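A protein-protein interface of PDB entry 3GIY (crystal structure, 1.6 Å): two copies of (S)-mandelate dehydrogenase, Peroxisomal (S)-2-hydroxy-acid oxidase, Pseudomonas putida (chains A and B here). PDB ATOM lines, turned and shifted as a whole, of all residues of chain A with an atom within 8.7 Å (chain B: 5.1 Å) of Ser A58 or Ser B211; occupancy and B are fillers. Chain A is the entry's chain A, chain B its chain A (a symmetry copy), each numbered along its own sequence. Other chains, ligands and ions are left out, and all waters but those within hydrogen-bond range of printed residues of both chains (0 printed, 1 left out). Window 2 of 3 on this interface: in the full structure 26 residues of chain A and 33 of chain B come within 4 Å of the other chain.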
ATOM      1  N   LEU A  54       2.730  23.742   8.609  1.00  0.00           N
ATOM      2  CA  LEU A  54       2.542  25.123   9.037  1.00  0.00           C
ATOM      3  C   LEU A  54       1.167  25.428   9.622  1.00  0.00           C
ATOM      4  O   LEU A  54       0.577  26.487   9.379  1.00  0.00           O
ATOM      5  CB  LEU A  54       2.872  26.062   7.878  1.00  0.00           C
ATOM      6  CG  LEU A  54       4.371  26.002   7.552  1.00  0.00           C
ATOM      7  CD1 LEU A  54       4.643  26.633   6.206  1.00  0.00           C
ATOM      8  CD2 LEU A  54       5.167  26.704   8.644  1.00  0.00           C
ATOM      9  N   VAL A  55       0.671  24.474  10.404  1.00  0.00           N
ATOM     10  CA  VAL A  55      -0.603  24.595  11.097  1.00  0.00           C
ATOM     11  C   VAL A  55      -0.240  24.659  12.575  1.00  0.00           C
ATOM     12  O   VAL A  55       0.623  23.910  13.035  1.00  0.00           O
ATOM     13  CB  VAL A  55      -1.501  23.361  10.878  1.00  0.00           C
ATOM     14  CG1 VAL A  55      -2.786  23.507  11.690  1.00  0.00           C
ATOM     15  CG2 VAL A  55      -1.804  23.190   9.405  1.00  0.00           C
ATOM     16  N   ASP A  56      -0.881  25.562  13.311  1.00  0.00           N
ATOM     17  CA  ASP A  56      -0.615  25.699  14.736  1.00  0.00           C
ATOM     18  C   ASP A  56      -1.250  24.529  15.481  1.00  0.00           C
ATOM     19  O   ASP A  56      -2.474  24.430  15.583  1.00  0.00           O
ATOM     20  CB  ASP A  56      -1.161  27.043  15.245  1.00  0.00           C
ATOM     21  CG  ASP A  56      -1.154  27.151  16.764  1.00  0.00           C
ATOM     22  OD1 ASP A  56      -0.394  26.407  17.419  1.00  0.00           O
ATOM     23  OD2 ASP A  56      -1.906  27.992  17.308  1.00  0.00           O
ATOM     24  N   VAL A  57      -0.409  23.627  15.978  1.00  0.00           N
ATOM     25  CA  VAL A  57      -0.888  22.464  16.717  1.00  0.00           C
ATOM     26  C   VAL A  57      -0.377  22.496  18.154  1.00  0.00           C
ATOM     27  O   VAL A  57      -0.195  21.455  18.782  1.00  0.00           O
ATOM     28  CB  VAL A  57      -0.449  21.128  16.043  1.00  0.00           C
ATOM     29  CG1 VAL A  57      -1.049  21.033  14.643  1.00  0.00           C
ATOM     30  CG2 VAL A  57       1.070  21.034  15.985  1.00  0.00           C
ATOM     31  N   SER A  58      -0.149  23.702  18.669  1.00  0.00           N
ATOM     32  CA  SER A  58       0.334  23.875  20.035  1.00  0.00           C
ATOM     33  C   SER A  58      -0.777  23.575  21.030  1.00  0.00           C
ATOM     34  O   SER A  58      -0.518  23.338  22.208  1.00  0.00           O
ATOM     35  CB  SER A  58       0.833  25.306  20.252  1.00  0.00           C
ATOM     36  OG  SER A  58      -0.203  26.237  20.013  1.00  0.00           O
ATOM     37  N   ARG A  59      -2.015  23.593  20.548  1.00  0.00           N
ATOM     38  CA  ARG A  59      -3.176  23.319  21.388  1.00  0.00           C
ATOM     39  C   ARG A  59      -4.053  22.290  20.677  1.00  0.00           C
ATOM     40  O   ARG A  59      -4.826  22.635  19.779  1.00  0.00           O
ATOM     41  CB  ARG A  59      -3.963  24.612  21.627  1.00  0.00           C
ATOM     42  CG  ARG A  59      -3.135  25.716  22.278  1.00  0.00           C
ATOM     43  CD  ARG A  59      -3.827  27.070  22.205  1.00  0.00           C
ATOM     44  NE  ARG A  59      -3.083  28.105  22.924  1.00  0.00           N
ATOM     45  CZ  ARG A  59      -1.850  28.508  22.618  1.00  0.00           C
ATOM     46  NH1 ARG A  59      -1.200  27.969  21.598  1.00  0.00           N
ATOM     47  NH2 ARG A  59      -1.266  29.456  23.336  1.00  0.00           N
ATOM     48  N   ARG A  60      -3.930  21.030  21.084  1.00  0.00           N
ATOM     49  CA  ARG A  60      -4.688  19.944  20.464  1.00  0.00           C
ATOM     50  C   ARG A  60      -5.787  19.398  21.370  1.00  0.00           C
ATOM     51  O   ARG A  60      -5.677  19.459  22.593  1.00  0.00           O
ATOM     52  CB  ARG A  60      -3.729  18.817  20.070  1.00  0.00           C
ATOM     53  CG  ARG A  60      -2.524  19.302  19.274  1.00  0.00           C
ATOM     54  CD  ARG A  60      -1.575  18.163  18.929  1.00  0.00           C
ATOM     55  NE  ARG A  60      -0.823  17.646  20.078  1.00  0.00           N
ATOM     56  CZ  ARG A  60       0.218  18.252  20.649  1.00  0.00           C
ATOM     57  NH1 ARG A  60       0.659  19.418  20.194  1.00  0.00           N
ATOM     58  NH2 ARG A  60       0.833  17.680  21.676  1.00  0.00           N
ATOM     59  N   SER A  61      -6.841  18.858  20.761  1.00  0.00           N
ATOM     60  CA  SER A  61      -7.962  18.301  21.513  1.00  0.00           C
ATOM     61  C   SER A  61      -8.385  16.944  20.952  1.00  0.00           C
ATOM     62  O   SER A  61      -8.618  16.806  19.751  1.00  0.00           O
ATOM     63  CB  SER A  61      -9.155  19.264  21.479  1.00  0.00           C
ATOM     64  OG  SER A  61     -10.248  18.759  22.231  1.00  0.00           O
ATOM     65  N   ASP A 334      -2.554  11.597  19.984  1.00  0.00           N
ATOM     66  CA  ASP A 334      -2.215  13.011  20.126  1.00  0.00           C
ATOM     67  C   ASP A 334      -1.020  13.387  19.252  1.00  0.00           C
ATOM     68  O   ASP A 334      -1.044  14.390  18.529  1.00  0.00           O
ATOM     69  CB  ASP A 334      -1.887  13.329  21.587  1.00  0.00           C
ATOM     70  CG  ASP A 334      -1.436  14.767  21.781  1.00  0.00           C
ATOM     71  OD1 ASP A 334      -2.256  15.687  21.584  1.00  0.00           O
ATOM     72  OD2 ASP A 334      -0.258  14.981  22.122  1.00  0.00           O
ATOM     73  N   ALA A 338      -0.857  15.871  15.793  1.00  0.00           N
ATOM     74  CA  ALA A 338       0.091  16.971  15.678  1.00  0.00           C
ATOM     75  C   ALA A 338       0.940  16.859  14.408  1.00  0.00           C
ATOM     76  O   ALA A 338       1.124  17.840  13.682  1.00  0.00           O
ATOM     77  CB  ALA A 338       0.996  17.009  16.904  1.00  0.00           C
ATOM     78  N   CYS A 342      -3.574  18.248  12.344  1.00  0.00           N
ATOM     79  CA  CYS A 342      -4.999  18.297  12.670  1.00  0.00           C
ATOM     80  C   CYS A 342      -5.151  18.336  14.194  1.00  0.00           C
ATOM     81  O   CYS A 342      -5.459  17.325  14.834  1.00  0.00           O
ATOM     82  CB  CYS A 342      -5.724  17.079  12.086  1.00  0.00           C
ATOM     83  SG  CYS A 342      -7.532  17.175  12.177  1.00  0.00           S
ATOM     84  N   PRO A 343      -4.957  19.527  14.791  1.00  0.00           N
ATOM     85  CA  PRO A 343      -5.046  19.758  16.238  1.00  0.00           C
ATOM     86  C   PRO A 343      -6.330  19.302  16.927  1.00  0.00           C
ATOM     87  O   PRO A 343      -6.284  18.842  18.073  1.00  0.00           O
ATOM     88  CB  PRO A 343      -4.809  21.266  16.363  1.00  0.00           C
ATOM     89  CG  PRO A 343      -5.372  21.801  15.084  1.00  0.00           C
ATOM     90  CD  PRO A 343      -4.836  20.810  14.071  1.00  0.00           C
ATOM     91  N   ARG B 135      10.888  32.216  18.954  1.00  0.00           N
ATOM     92  CA  ARG B 135      10.922  33.182  17.854  1.00  0.00           C
ATOM     93  C   ARG B 135      12.125  34.121  17.928  1.00  0.00           C
ATOM     94  O   ARG B 135      12.847  34.304  16.945  1.00  0.00           O
ATOM     95  CB  ARG B 135       9.631  34.011  17.829  1.00  0.00           C
ATOM     96  CG  ARG B 135       8.353  33.196  17.634  1.00  0.00           C
ATOM     97  CD  ARG B 135       8.395  32.382  16.351  1.00  0.00           C
ATOM     98  NE  ARG B 135       7.161  31.629  16.124  1.00  0.00           N
ATOM     99  CZ  ARG B 135       6.014  32.166  15.715  1.00  0.00           C
ATOM    100  NH1 ARG B 135       5.936  33.469  15.482  1.00  0.00           N
ATOM    101  NH2 ARG B 135       4.945  31.400  15.533  1.00  0.00           N
ATOM    102  N   ASP B 209       8.518  24.944  18.558  1.00  0.00           N
ATOM    103  CA  ASP B 209       7.346  25.794  18.421  1.00  0.00           C
ATOM    104  C   ASP B 209       6.302  25.118  17.530  1.00  0.00           C
ATOM    105  O   ASP B 209       6.382  25.175  16.304  1.00  0.00           O
ATOM    106  CB  ASP B 209       7.777  27.143  17.843  1.00  0.00           C
ATOM    107  CG  ASP B 209       6.645  28.133  17.764  1.00  0.00           C
ATOM    108  OD1 ASP B 209       5.686  28.001  18.553  1.00  0.00           O
ATOM    109  OD2 ASP B 209       6.725  29.048  16.918  1.00  0.00           O
ATOM    110  N   ALA B 210       5.327  24.474  18.167  1.00  0.00           N
ATOM    111  CA  ALA B 210       4.271  23.766  17.457  1.00  0.00           C
ATOM    112  C   ALA B 210       3.210  24.708  16.888  1.00  0.00           C
ATOM    113  O   ALA B 210       2.281  24.271  16.205  1.00  0.00           O
ATOM    114  CB  ALA B 210       3.620  22.756  18.388  1.00  0.00           C
ATOM    115  N   SER B 211       3.352  26.000  17.164  1.00  0.00           N
ATOM    116  CA  SER B 211       2.391  26.989  16.687  1.00  0.00           C
ATOM    117  C   SER B 211       2.863  27.719  15.435  1.00  0.00           C
ATOM    118  O   SER B 211       2.106  28.493  14.847  1.00  0.00           O
ATOM    119  CB  SER B 211       2.114  28.026  17.778  1.00  0.00           C
ATOM    120  OG  SER B 211       3.182  28.953  17.869  1.00  0.00           O
ATOM    121  N   PHE B 212       4.108  27.486  15.031  1.00  0.00           N
ATOM    122  CA  PHE B 212       4.645  28.162  13.854  1.00  0.00           C
ATOM    123  C   PHE B 212       3.760  27.847  12.654  1.00  0.00           C
ATOM    124  O   PHE B 212       3.714  26.705  12.185  1.00  0.00           O
ATOM    125  CB  PHE B 212       6.094  27.735  13.601  1.00  0.00           C
ATOM    126  CG  PHE B 212       6.878  28.727  12.785  1.00  0.00           C
ATOM    127  CD1 PHE B 212       6.878  28.667  11.395  1.00  0.00           C
ATOM    128  CD2 PHE B 212       7.573  29.759  13.410  1.00  0.00           C
ATOM    129  CE1 PHE B 212       7.554  29.620  10.641  1.00  0.00           C
ATOM    130  CE2 PHE B 212       8.254  30.720  12.662  1.00  0.00           C
ATOM    131  CZ  PHE B 212       8.242  30.650  11.275  1.00  0.00           C
ATOM    132  N   ASN B 213       3.051  28.871  12.179  1.00  0.00           N
ATOM    133  CA  ASN B 213       2.121  28.741  11.061  1.00  0.00           C
ATOM    134  C   ASN B 213       2.468  29.609   9.859  1.00  0.00           C
ATOM    135  O   ASN B 213       3.576  30.141   9.762  1.00  0.00           O
ATOM    136  CB  ASN B 213       0.698  29.075  11.521  1.00  0.00           C
ATOM    137  CG  ASN B 213       0.617  30.409  12.247  1.00  0.00           C
ATOM    138  OD1 ASN B 213       1.278  31.376  11.869  1.00  0.00           O
ATOM    139  ND2 ASN B 213      -0.203  30.467  13.289  1.00  0.00           N
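No position is printed for both chains.
Of the 8 pairs that touch across the chains among the printed residues, none has its exchanged pair printed and touching as well.
Hydrophobic or aromatic side chains of chain A that line the printed part of chain B: Leu A54 and Val A57.
Of the 6 printed residues of chain B, 4 touch a printed residue of chain A.
Hydrophobic or aromatic side chains of chain B within 4 Å of the printed part of chain A: Ala B210 and Phe B212.
Along chain B the printed residues that touch a printed residue of chain A span positions 210 to 213.
Among the printed residues, merely in contact across the chains: Leu A54 with Phe B212 (3.7 Å), Leu A54 with Asn B213 (3.2 Å), Val A55 with Ala B210 (3.6 Å), Asp A56 with Ala B210 (3.5 Å), Asp A56 with Ser B211 (2.9 Å), Ser A58 with Ala B210 (3.5 Å) and Ser A58 with Ser B211 (3.7 Å).
Printed residues of chain B within 4 Å of Val A55: Ala B210.
Of the printed residues of chain B, Val A57 touches Ala B210.
Of chain B, only Ala B210 (3.5 Å) and Ser B211 (3.7 Å) come within 4 Å of Ser A58.
Arg A59 touches none of the printed residues of chain B.
Of the printed residues of chain A, Ala B210 touches Val A55, Asp A56, Val A57 and Ser A58.
Ser B211 touches just these residues of chain A: Asp A56 and Ser A58.
Of the printed residues of chain A, Phe B212 touches Leu A54 (3.7 Å).
The nearest printed residue of chain B that does not touch Ser A58 is Asp B209 (5.8 Å).
The nearest printed residue of chain B that does not touch Val A55 is Phe B212 (4.2 Å).
O of Val A57 is in hydrogen-bond range of NH1 of Arg A60 (2.6 Å).
OD1 of Asp B209 lies within hydrogen-bond range of OG of Ser B211 (2.8 Å).
O of Ser B211 sits at hydrogen-bond distance from ND2 of Asn B213 (3.4 Å).
The side-chain hydroxyl (OG) of Ser A58 sits at hydrogen-bond distance from the guanidinium group (NH1) of Arg A59 (2.6 Å).
OD1 of Asp A56 is in hydrogen-bond range of OG of Ser A58 (2.6 Å).
The backbone carbonyl oxygen of Ala B210 is in hydrogen-bond range of the backbone NH of Val A57 (2.8 Å).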
